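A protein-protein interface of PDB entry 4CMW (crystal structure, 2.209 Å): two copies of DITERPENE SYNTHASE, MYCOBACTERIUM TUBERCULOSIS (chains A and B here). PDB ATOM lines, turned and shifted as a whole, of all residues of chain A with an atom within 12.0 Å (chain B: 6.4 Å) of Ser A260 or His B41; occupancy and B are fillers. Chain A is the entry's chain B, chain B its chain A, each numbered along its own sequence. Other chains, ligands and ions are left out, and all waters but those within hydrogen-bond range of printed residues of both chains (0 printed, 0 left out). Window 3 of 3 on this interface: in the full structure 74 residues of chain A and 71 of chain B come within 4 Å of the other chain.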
ATOM      1  N   PRO A 255      33.996 -12.601 -19.795  1.00  0.00           N
ATOM      2  CA  PRO A 255      33.711 -11.747 -20.953  1.00  0.00           C
ATOM      3  C   PRO A 255      32.385 -10.978 -20.844  1.00  0.00           C
ATOM      4  O   PRO A 255      31.512 -11.354 -20.061  1.00  0.00           O
ATOM      5  CB  PRO A 255      33.661 -12.752 -22.111  1.00  0.00           C
ATOM      6  CG  PRO A 255      33.215 -14.028 -21.483  1.00  0.00           C
ATOM      7  CD  PRO A 255      33.810 -14.034 -20.098  1.00  0.00           C
ATOM      8  N   LYS A 256      32.258  -9.920 -21.644  1.00  0.00           N
ATOM      9  CA  LYS A 256      31.031  -9.146 -21.757  1.00  0.00           C
ATOM     10  C   LYS A 256      29.934  -9.997 -22.360  1.00  0.00           C
ATOM     11  O   LYS A 256      30.214 -10.959 -23.060  1.00  0.00           O
ATOM     12  CB  LYS A 256      31.256  -7.907 -22.628  1.00  0.00           C
ATOM     13  CG  LYS A 256      32.020  -6.805 -21.931  1.00  0.00           C
ATOM     14  CD  LYS A 256      32.457  -5.711 -22.900  1.00  0.00           C
ATOM     15  CE  LYS A 256      31.300  -5.207 -23.752  1.00  0.00           C
ATOM     16  NZ  LYS A 256      31.719  -4.172 -24.746  1.00  0.00           N
ATOM     17  N   PRO A 257      28.671  -9.657 -22.077  1.00  0.00           N
ATOM     18  CA  PRO A 257      27.552 -10.470 -22.566  1.00  0.00           C
ATOM     19  C   PRO A 257      27.535 -10.598 -24.096  1.00  0.00           C
ATOM     20  O   PRO A 257      27.775  -9.620 -24.806  1.00  0.00           O
ATOM     21  CB  PRO A 257      26.310  -9.712 -22.059  1.00  0.00           C
ATOM     22  CG  PRO A 257      26.798  -8.333 -21.693  1.00  0.00           C
ATOM     23  CD  PRO A 257      28.208  -8.549 -21.224  1.00  0.00           C
ATOM     24  N   ASP A 258      27.279 -11.807 -24.586  1.00  0.00           N
ATOM     25  CA  ASP A 258      27.163 -12.067 -26.019  1.00  0.00           C
ATOM     26  C   ASP A 258      25.711 -12.413 -26.338  1.00  0.00           C
ATOM     27  O   ASP A 258      25.304 -13.569 -26.237  1.00  0.00           O
ATOM     28  CB  ASP A 258      28.092 -13.223 -26.413  1.00  0.00           C
ATOM     29  CG  ASP A 258      28.108 -13.488 -27.914  1.00  0.00           C
ATOM     30  OD1 ASP A 258      27.655 -12.615 -28.688  1.00  0.00           O
ATOM     31  OD2 ASP A 258      28.586 -14.569 -28.320  1.00  0.00           O
ATOM     32  N   TYR A 259      24.932 -11.405 -26.718  1.00  0.00           N
ATOM     33  CA  TYR A 259      23.495 -11.586 -26.895  1.00  0.00           C
ATOM     34  C   TYR A 259      23.176 -12.538 -28.041  1.00  0.00           C
ATOM     35  O   TYR A 259      22.186 -13.261 -27.990  1.00  0.00           O
ATOM     36  CB  TYR A 259      22.781 -10.239 -27.081  1.00  0.00           C
ATOM     37  CG  TYR A 259      23.131  -9.246 -26.001  1.00  0.00           C
ATOM     38  CD1 TYR A 259      22.742  -9.456 -24.681  1.00  0.00           C
ATOM     39  CD2 TYR A 259      23.867  -8.103 -26.296  1.00  0.00           C
ATOM     40  CE1 TYR A 259      23.080  -8.554 -23.681  1.00  0.00           C
ATOM     41  CE2 TYR A 259      24.210  -7.198 -25.302  1.00  0.00           C
ATOM     42  CZ  TYR A 259      23.812  -7.427 -24.001  1.00  0.00           C
ATOM     43  OH  TYR A 259      24.150  -6.527 -23.018  1.00  0.00           O
ATOM     44  N   SER A 260      24.025 -12.536 -29.064  1.00  0.00           N
ATOM     45  CA  SER A 260      23.821 -13.383 -30.237  1.00  0.00           C
ATOM     46  C   SER A 260      23.929 -14.871 -29.902  1.00  0.00           C
ATOM     47  O   SER A 260      23.291 -15.708 -30.536  1.00  0.00           O
ATOM     48  CB  SER A 260      24.837 -13.029 -31.329  1.00  0.00           C
ATOM     49  OG  SER A 260      24.983 -11.624 -31.466  1.00  0.00           O
ATOM     50  N   ALA A 261      24.721 -15.191 -28.887  1.00  0.00           N
ATOM     51  CA  ALA A 261      24.941 -16.579 -28.501  1.00  0.00           C
ATOM     52  C   ALA A 261      23.936 -17.047 -27.461  1.00  0.00           C
ATOM     53  O   ALA A 261      24.037 -18.156 -26.949  1.00  0.00           O
ATOM     54  CB  ALA A 261      26.355 -16.762 -27.982  1.00  0.00           C
ATOM     55  N   MET A 262      22.967 -16.199 -27.142  1.00  0.00           N
ATOM     56  CA  MET A 262      21.999 -16.520 -26.101  1.00  0.00           C
ATOM     57  C   MET A 262      20.796 -17.223 -26.709  1.00  0.00           C
ATOM     58  O   MET A 262      20.415 -16.943 -27.844  1.00  0.00           O
ATOM     59  CB  MET A 262      21.564 -15.252 -25.350  1.00  0.00           C
ATOM     60  CG  MET A 262      22.671 -14.626 -24.508  1.00  0.00           C
ATOM     61  SD  MET A 262      22.237 -13.036 -23.748  1.00  0.00           S
ATOM     62  CE  MET A 262      20.959 -13.518 -22.599  1.00  0.00           C
ATOM     63  N   SER A 263      20.208 -18.148 -25.960  1.00  0.00           N
ATOM     64  CA  SER A 263      19.062 -18.889 -26.462  1.00  0.00           C
ATOM     65  C   SER A 263      17.869 -17.960 -26.579  1.00  0.00           C
ATOM     66  O   SER A 263      17.869 -16.867 -26.016  1.00  0.00           O
ATOM     67  CB  SER A 263      18.723 -20.055 -25.536  1.00  0.00           C
ATOM     68  OG  SER A 263      18.118 -19.587 -24.344  1.00  0.00           O
ATOM     69  N   ALA A 264      16.854 -18.403 -27.315  1.00  0.00           N
ATOM     70  CA  ALA A 264      15.639 -17.623 -27.515  1.00  0.00           C
ATOM     71  C   ALA A 264      14.961 -17.341 -26.181  1.00  0.00           C
ATOM     72  O   ALA A 264      14.401 -16.259 -25.956  1.00  0.00           O
ATOM     73  CB  ALA A 264      14.693 -18.357 -28.442  1.00  0.00           C
ATOM     74  N   ASP A 265      15.033 -18.327 -25.293  1.00  0.00           N
ATOM     75  CA  ASP A 265      14.364 -18.255 -24.002  1.00  0.00           C
ATOM     76  C   ASP A 265      15.033 -17.268 -23.032  1.00  0.00           C
ATOM     77  O   ASP A 265      14.346 -16.548 -22.301  1.00  0.00           O
ATOM     78  CB  ASP A 265      14.282 -19.655 -23.395  1.00  0.00           C
ATOM     79  CG  ASP A 265      13.549 -20.631 -24.298  1.00  0.00           C
ATOM     80  OD1 ASP A 265      12.484 -20.260 -24.835  1.00  0.00           O
ATOM     81  OD2 ASP A 265      14.043 -21.762 -24.483  1.00  0.00           O
ATOM     82  N   GLN A 266      16.365 -17.220 -23.040  1.00  0.00           N
ATOM     83  CA  GLN A 266      17.110 -16.258 -22.226  1.00  0.00           C
ATOM     84  C   GLN A 266      16.762 -14.822 -22.635  1.00  0.00           C
ATOM     85  O   GLN A 266      16.441 -13.952 -21.789  1.00  0.00           O
ATOM     86  CB  GLN A 266      18.611 -16.488 -22.397  1.00  0.00           C
ATOM     87  CG  GLN A 266      19.169 -17.655 -21.608  1.00  0.00           C
ATOM     88  CD  GLN A 266      20.579 -18.013 -22.040  1.00  0.00           C
ATOM     89  OE1 GLN A 266      20.905 -17.965 -23.227  1.00  0.00           O
ATOM     90  NE2 GLN A 266      21.422 -18.378 -21.079  1.00  0.00           N
ATOM     91  N   LEU A 267      16.771 -14.609 -23.950  1.00  0.00           N
ATOM     92  CA  LEU A 267      16.405 -13.328 -24.533  1.00  0.00           C
ATOM     93  C   LEU A 267      14.980 -12.997 -24.133  1.00  0.00           C
ATOM     94  O   LEU A 267      14.673 -11.853 -23.846  1.00  0.00           O
ATOM     95  CB  LEU A 267      16.541 -13.350 -26.060  1.00  0.00           C
ATOM     96  CG  LEU A 267      17.948 -13.440 -26.660  1.00  0.00           C
ATOM     97  CD1 LEU A 267      17.891 -13.265 -28.168  1.00  0.00           C
ATOM     98  CD2 LEU A 267      18.892 -12.424 -26.035  1.00  0.00           C
ATOM     99  N   ASN A 268      14.115 -14.007 -24.119  1.00  0.00           N
ATOM    100  CA  ASN A 268      12.742 -13.826 -23.652  1.00  0.00           C
ATOM    101  C   ASN A 268      12.652 -13.360 -22.201  1.00  0.00           C
ATOM    102  O   ASN A 268      11.851 -12.487 -21.878  1.00  0.00           O
ATOM    103  CB  ASN A 268      11.932 -15.103 -23.848  1.00  0.00           C
ATOM    104  CG  ASN A 268      11.508 -15.291 -25.275  1.00  0.00           C
ATOM    105  OD1 ASN A 268      11.281 -14.315 -25.992  1.00  0.00           O
ATOM    106  ND2 ASN A 268      11.404 -16.545 -25.707  1.00  0.00           N
ATOM    107  N   VAL A 269      13.453 -13.960 -21.325  1.00  0.00           N
ATOM    108  CA  VAL A 269      13.500 -13.526 -19.928  1.00  0.00           C
ATOM    109  C   VAL A 269      13.918 -12.061 -19.807  1.00  0.00           C
ATOM    110  O   VAL A 269      13.241 -11.268 -19.129  1.00  0.00           O
ATOM    111  CB  VAL A 269      14.436 -14.410 -19.072  1.00  0.00           C
ATOM    112  CG1 VAL A 269      14.841 -13.685 -17.795  1.00  0.00           C
ATOM    113  CG2 VAL A 269      13.769 -15.741 -18.753  1.00  0.00           C
ATOM    114  N   LEU A 270      15.001 -11.691 -20.495  1.00  0.00           N
ATOM    115  CA  LEU A 270      15.450 -10.292 -20.457  1.00  0.00           C
ATOM    116  C   LEU A 270      14.379  -9.337 -20.992  1.00  0.00           C
ATOM    117  O   LEU A 270      14.036  -8.339 -20.351  1.00  0.00           O
ATOM    118  CB  LEU A 270      16.759 -10.113 -21.234  1.00  0.00           C
ATOM    119  CG  LEU A 270      17.991 -10.765 -20.595  1.00  0.00           C
ATOM    120  CD1 LEU A 270      19.214 -10.635 -21.480  1.00  0.00           C
ATOM    121  CD2 LEU A 270      18.264 -10.130 -19.234  1.00  0.00           C
ATOM    122  N   ARG A 271      13.852  -9.668 -22.167  1.00  0.00           N
ATOM    123  CA  ARG A 271      12.829  -8.886 -22.857  1.00  0.00           C
ATOM    124  C   ARG A 271      11.582  -8.668 -21.982  1.00  0.00           C
ATOM    125  O   ARG A 271      11.090  -7.539 -21.850  1.00  0.00           O
ATOM    126  CB  ARG A 271      12.464  -9.609 -24.161  1.00  0.00           C
ATOM    127  CG  ARG A 271      11.802  -8.749 -25.216  1.00  0.00           C
ATOM    128  CD  ARG A 271      11.492  -9.554 -26.477  1.00  0.00           C
ATOM    129  NE  ARG A 271      12.681  -9.838 -27.282  1.00  0.00           N
ATOM    130  CZ  ARG A 271      13.191 -11.051 -27.479  1.00  0.00           C
ATOM    131  NH1 ARG A 271      12.618 -12.119 -26.940  1.00  0.00           N
ATOM    132  NH2 ARG A 271      14.270 -11.198 -28.235  1.00  0.00           N
ATOM    133  N   ASN A 272      11.095  -9.746 -21.366  1.00  0.00           N
ATOM    134  CA  ASN A 272       9.934  -9.678 -20.477  1.00  0.00           C
ATOM    135  C   ASN A 272      10.214  -8.842 -19.230  1.00  0.00           C
ATOM    136  O   ASN A 272       9.422  -7.956 -18.886  1.00  0.00           O
ATOM    137  CB  ASN A 272       9.493 -11.084 -20.061  1.00  0.00           C
ATOM    138  CG  ASN A 272       8.827 -11.848 -21.192  1.00  0.00           C
ATOM    139  OD1 ASN A 272       8.665 -11.335 -22.301  1.00  0.00           O
ATOM    140  ND2 ASN A 272       8.455 -13.091 -20.918  1.00  0.00           N
ATOM    141  N   TYR A 274      12.470  -6.446 -18.777  1.00  0.00           N
ATOM    142  CA  TYR A 274      12.625  -5.035 -19.101  1.00  0.00           C
ATOM    143  C   TYR A 274      11.308  -4.432 -19.553  1.00  0.00           C
ATOM    144  O   TYR A 274      11.081  -3.231 -19.389  1.00  0.00           O
ATOM    145  CB  TYR A 274      13.695  -4.823 -20.165  1.00  0.00           C
ATOM    146  CG  TYR A 274      15.073  -5.219 -19.711  1.00  0.00           C
ATOM    147  CD1 TYR A 274      15.413  -5.189 -18.361  1.00  0.00           C
ATOM    148  CD2 TYR A 274      16.044  -5.611 -20.628  1.00  0.00           C
ATOM    149  CE1 TYR A 274      16.680  -5.540 -17.937  1.00  0.00           C
ATOM    150  CE2 TYR A 274      17.317  -5.966 -20.207  1.00  0.00           C
ATOM    151  CZ  TYR A 274      17.628  -5.930 -18.860  1.00  0.00           C
ATOM    152  OH  TYR A 274      18.893  -6.285 -18.435  1.00  0.00           O
ATOM    153  N   ARG A 275      10.437  -5.249 -20.139  1.00  0.00           N
ATOM    154  CA  ARG A 275       9.165  -4.709 -20.600  1.00  0.00           C
ATOM    155  C   ARG A 275       8.159  -4.448 -19.466  1.00  0.00           C
ATOM    156  O   ARG A 275       7.449  -3.438 -19.491  1.00  0.00           O
ATOM    157  CB  ARG A 275       8.554  -5.606 -21.682  1.00  0.00           C
ATOM    158  CG  ARG A 275       9.136  -5.372 -23.085  1.00  0.00           C
ATOM    159  CD  ARG A 275       8.801  -6.517 -24.040  1.00  0.00           C
ATOM    160  NE  ARG A 275       9.372  -6.308 -25.367  1.00  0.00           N
ATOM    161  CZ  ARG A 275       8.993  -6.974 -26.454  1.00  0.00           C
ATOM    162  NH1 ARG A 275       8.038  -7.889 -26.369  1.00  0.00           N
ATOM    163  NH2 ARG A 275       9.558  -6.721 -27.629  1.00  0.00           N
ATOM    164  N   THR B  36      22.397   0.259 -25.056  1.00  0.00           N
ATOM    165  CA  THR B  36      21.761   0.260 -26.373  1.00  0.00           C
ATOM    166  C   THR B  36      22.008  -1.029 -27.194  1.00  0.00           C
ATOM    167  O   THR B  36      21.131  -1.448 -27.944  1.00  0.00           O
ATOM    168  CB  THR B  36      22.122   1.525 -27.195  1.00  0.00           C
ATOM    169  OG1 THR B  36      23.545   1.637 -27.319  1.00  0.00           O
ATOM    170  CG2 THR B  36      21.535   2.811 -26.536  1.00  0.00           C
ATOM    171  N   ARG B  37      23.183  -1.655 -27.066  1.00  0.00           N
ATOM    172  CA  ARG B  37      23.423  -2.961 -27.711  1.00  0.00           C
ATOM    173  C   ARG B  37      22.379  -3.992 -27.260  1.00  0.00           C
ATOM    174  O   ARG B  37      21.762  -4.698 -28.077  1.00  0.00           O
ATOM    175  CB  ARG B  37      24.829  -3.494 -27.420  1.00  0.00           C
ATOM    176  CG  ARG B  37      25.932  -2.925 -28.290  1.00  0.00           C
ATOM    177  CD  ARG B  37      27.134  -3.883 -28.442  1.00  0.00           C
ATOM    178  NE  ARG B  37      27.409  -4.737 -27.280  1.00  0.00           N
ATOM    179  CZ  ARG B  37      27.203  -6.056 -27.241  1.00  0.00           C
ATOM    180  NH1 ARG B  37      26.723  -6.686 -28.304  1.00  0.00           N
ATOM    181  NH2 ARG B  37      27.488  -6.754 -26.145  1.00  0.00           N
ATOM    182  N   ARG B  38      22.195  -4.072 -25.945  1.00  0.00           N
ATOM    183  CA  ARG B  38      21.259  -5.012 -25.350  1.00  0.00           C
ATOM    184  C   ARG B  38      19.842  -4.709 -25.823  1.00  0.00           C
ATOM    185  O   ARG B  38      19.114  -5.603 -26.295  1.00  0.00           O
ATOM    186  CB  ARG B  38      21.333  -4.920 -23.827  1.00  0.00           C
ATOM    187  CG  ARG B  38      20.585  -6.012 -23.098  1.00  0.00           C
ATOM    188  CD  ARG B  38      20.685  -5.821 -21.605  1.00  0.00           C
ATOM    189  NE  ARG B  38      22.083  -5.771 -21.190  1.00  0.00           N
ATOM    190  CZ  ARG B  38      22.495  -5.432 -19.972  1.00  0.00           C
ATOM    191  NH1 ARG B  38      21.612  -5.144 -19.027  1.00  0.00           N
ATOM    192  NH2 ARG B  38      23.789  -5.403 -19.696  1.00  0.00           N
ATOM    193  N   TRP B  39      19.467  -3.437 -25.726  1.00  0.00           N
ATOM    194  CA  TRP B  39      18.146  -3.021 -26.172  1.00  0.00           C
ATOM    195  C   TRP B  39      17.904  -3.422 -27.618  1.00  0.00           C
ATOM    196  O   TRP B  39      16.834  -3.916 -27.948  1.00  0.00           O
ATOM    197  CB  TRP B  39      17.939  -1.508 -26.029  1.00  0.00           C
ATOM    198  CG  TRP B  39      16.670  -1.079 -26.705  1.00  0.00           C
ATOM    199  CD1 TRP B  39      15.410  -1.111 -26.182  1.00  0.00           C
ATOM    200  CD2 TRP B  39      16.538  -0.566 -28.036  1.00  0.00           C
ATOM    201  NE1 TRP B  39      14.503  -0.651 -27.107  1.00  0.00           N
ATOM    202  CE2 TRP B  39      15.173  -0.311 -28.253  1.00  0.00           C
ATOM    203  CE3 TRP B  39      17.444  -0.294 -29.064  1.00  0.00           C
ATOM    204  CZ2 TRP B  39      14.691   0.195 -29.453  1.00  0.00           C
ATOM    205  CZ3 TRP B  39      16.964   0.211 -30.256  1.00  0.00           C
ATOM    206  CH2 TRP B  39      15.602   0.450 -30.441  1.00  0.00           C
ATOM    207  N   PHE B  40      18.908  -3.219 -28.465  1.00  0.00           N
ATOM    208  CA  PHE B  40      18.792  -3.525 -29.886  1.00  0.00           C
ATOM    209  C   PHE B  40      18.635  -5.020 -30.146  1.00  0.00           C
ATOM    210  O   PHE B  40      17.780  -5.436 -30.936  1.00  0.00           O
ATOM    211  CB  PHE B  40      19.988  -2.958 -30.657  1.00  0.00           C
ATOM    212  CG  PHE B  40      19.971  -3.281 -32.127  1.00  0.00           C
ATOM    213  CD1 PHE B  40      19.147  -2.579 -32.992  1.00  0.00           C
ATOM    214  CD2 PHE B  40      20.785  -4.279 -32.641  1.00  0.00           C
ATOM    215  CE1 PHE B  40      19.130  -2.870 -34.343  1.00  0.00           C
ATOM    216  CE2 PHE B  40      20.775  -4.577 -33.990  1.00  0.00           C
ATOM    217  CZ  PHE B  40      19.947  -3.869 -34.844  1.00  0.00           C
ATOM    218  N   HIS B  41      19.428  -5.832 -29.453  1.00  0.00           N
ATOM    219  CA  HIS B  41      19.281  -7.277 -29.588  1.00  0.00           C
ATOM    220  C   HIS B  41      17.943  -7.787 -29.055  1.00  0.00           C
ATOM    221  O   HIS B  41      17.476  -8.851 -29.473  1.00  0.00           O
ATOM    222  CB  HIS B  41      20.442  -8.033 -28.939  1.00  0.00           C
ATOM    223  CG  HIS B  41      21.662  -8.131 -29.803  1.00  0.00           C
ATOM    224  ND1 HIS B  41      22.682  -7.206 -29.764  1.00  0.00           N
ATOM    225  CD2 HIS B  41      22.022  -9.048 -30.733  1.00  0.00           C
ATOM    226  CE1 HIS B  41      23.619  -7.549 -30.628  1.00  0.00           C
ATOM    227  NE2 HIS B  41      23.243  -8.662 -31.231  1.00  0.00           N
ATOM    228  N   LEU B  42      17.334  -7.032 -28.140  1.00  0.00           N
ATOM    229  CA  LEU B  42      16.062  -7.450 -27.537  1.00  0.00           C
ATOM    230  C   LEU B  42      14.769  -6.958 -28.222  1.00  0.00           C
ATOM    231  O   LEU B  42      13.744  -7.640 -28.192  1.00  0.00           O
ATOM    232  CB  LEU B  42      16.030  -7.061 -26.062  1.00  0.00           C
ATOM    233  CG  LEU B  42      17.026  -7.767 -25.156  1.00  0.00           C
ATOM    234  CD1 LEU B  42      16.971  -7.148 -23.782  1.00  0.00           C
ATOM    235  CD2 LEU B  42      16.697  -9.251 -25.086  1.00  0.00           C
ATOM    236  N   GLU B  43      14.810  -5.769 -28.811  1.00  0.00           N
ATOM    237  CA  GLU B  43      13.597  -5.130 -29.316  1.00  0.00           C
ATOM    238  C   GLU B  43      13.581  -4.967 -30.827  1.00  0.00           C
ATOM    239  O   GLU B  43      12.561  -4.610 -31.414  1.00  0.00           O
ATOM    240  CB  GLU B  43      13.379  -3.774 -28.642  1.00  0.00           C
ATOM    241  CG  GLU B  43      13.191  -3.870 -27.144  1.00  0.00           C
ATOM    242  CD  GLU B  43      12.044  -4.789 -26.757  1.00  0.00           C
ATOM    243  OE1 GLU B  43      11.069  -4.884 -27.533  1.00  0.00           O
ATOM    244  OE2 GLU B  43      12.109  -5.408 -25.675  1.00  0.00           O
ATOM    245  N   CYS B  44      14.717  -5.227 -31.457  1.00  0.00           N
ATOM    246  CA  CYS B  44      14.792  -5.160 -32.904  1.00  0.00           C
ATOM    247  C   CYS B  44      15.171  -6.534 -33.456  1.00  0.00           C
ATOM    248  O   CYS B  44      15.423  -7.482 -32.698  1.00  0.00           O
ATOM    249  CB  CYS B  44      15.820  -4.112 -33.323  1.00  0.00           C
ATOM    250  SG  CYS B  44      15.487  -2.464 -32.633  1.00  0.00           S
ATOM    251  N   ASN B  45      15.213  -6.634 -34.776  1.00  0.00           N
ATOM    252  CA  ASN B  45      15.675  -7.847 -35.437  1.00  0.00           C
ATOM    253  C   ASN B  45      17.068  -7.545 -35.929  1.00  0.00           C
ATOM    254  O   ASN B  45      17.234  -6.867 -36.943  1.00  0.00           O
ATOM    255  CB  ASN B  45      14.759  -8.217 -36.608  1.00  0.00           C
ATOM    256  CG  ASN B  45      14.837  -9.689 -36.978  1.00  0.00           C
ATOM    257  OD1 ASN B  45      15.906 -10.301 -36.968  1.00  0.00           O
ATOM    258  ND2 ASN B  45      13.689 -10.267 -37.303  1.00  0.00           N
ATOM    259  N   PRO B  46      18.083  -8.025 -35.195  1.00  0.00           N
ATOM    260  CA  PRO B  46      19.464  -7.689 -35.549  1.00  0.00           C
ATOM    261  C   PRO B  46      19.810  -8.171 -36.950  1.00  0.00           C
ATOM    262  O   PRO B  46      20.761  -7.669 -37.545  1.00  0.00           O
ATOM    263  CB  PRO B  46      20.285  -8.447 -34.496  1.00  0.00           C
ATOM    264  CG  PRO B  46      19.337  -8.606 -33.330  1.00  0.00           C
ATOM    265  CD  PRO B  46      18.006  -8.841 -33.972  1.00  0.00           C
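The guanidinium group (NE) of Arg B38 is in hydrogen-bond range of the side-chain hydroxyl (OH) of Tyr A259 (2.9 Å). The guanidinium group (NH2) of Arg B37 is in hydrogen-bond range of the backbone carbonyl oxygen (O) of Pro A257, 3.2 Å away. NE2 of His B41 is in hydrogen-bond range of OG of Ser A260, at 3.4 Å. The guanidinium group of Arg B38 is in hydrogen-bond range of the side-chain hydroxyl of Tyr A274 (3.0 Å). The side-chain carboxylate of Glu B43 lies within salt-bridge range of the guanidinium group of Arg A275 (2.9 Å). O of Leu B42 is in hydrogen-bond range of NE of Arg A271, at 2.6 Å.
ND1 of His B41 sits at hydrogen-bond distance from O of Arg B37. The side-chain amide oxygen (OD1) of Asn A268 is in hydrogen-bond range of the guanidinium group (NH1) of Arg A271 (2.7 Å).
Tyr A259 touches Arg B37. CB of Tyr A259 touches CG of His B41, 3.6 Å away. CD2 of Leu B42 touches O of Leu A267, 3.5 Å away. CB of Leu A270 touches CD1 of Leu B42, at 3.9 Å. CG of Arg A271 touches OE2 of Glu B43 (3.4 Å). Tyr A274 touches Leu B42.
Pro A255 touches none of the printed residues of chain B. Of the printed residues of chain B, Pro A257 touches Arg B37. Of the printed residues of chain B, Leu A270 touches Leu B42 (3.9 Å). Of the printed residues of chain B, Arg A271 touches Leu B42 and Glu B43. Of the printed residues of chain B, Tyr A274 touches Arg B38 and Leu B42. Of the printed residues of chain B, Arg A275 touches Glu B43. Thr B36 touches none of the printed residues of chain A. Printed residues of chain A within 4 Å of Arg B37: Pro A257 (3.2 Å) and Tyr A259 (3.4 Å). No residue of chain A comes within 4 Å of Phe B40. Of chain A, only Tyr A259 and Ser A260 come within 4 Å of His B41. Leu B42 touches just these residues of chain A: Leu A267 (3.5 Å), Leu A270 (3.9 Å), Arg A271 (2.6 Å) and Tyr A274 (3.6 Å). Of chain A, only Arg A271 and Arg A275 come within 4 Å of Glu B43. No residue of chain A comes within 4 Å of Cys B44. No residue of chain A comes within 4 Å of Pro B46. The nearest residue of chain B that does not touch Ser A260 is Arg B37 (6.1 Å). The nearest printed residue of chain B that does not touch Pro A257 is Arg B38 (4.7 Å).
Of the 20 printed residues of chain A, 8 touch a printed residue of chain B. Hydrophobic or aromatic side chains of chain A within 4 Å of the printed part of chain B: Tyr A259, Leu A267, Leu A270 and Tyr A274. Of the 11 printed residues of chain B, 5 touch a printed residue of chain A. Hydrophobic or aromatic side chains of chain B that line the printed part of chain A: His B41 and Leu B42. Among the printed residues, 12 pairs touch across the chains.
No position is printed for both chains. Of the 12 pairs that touch across the chains among the printed residues, none has its exchanged pair printed and touching as well.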
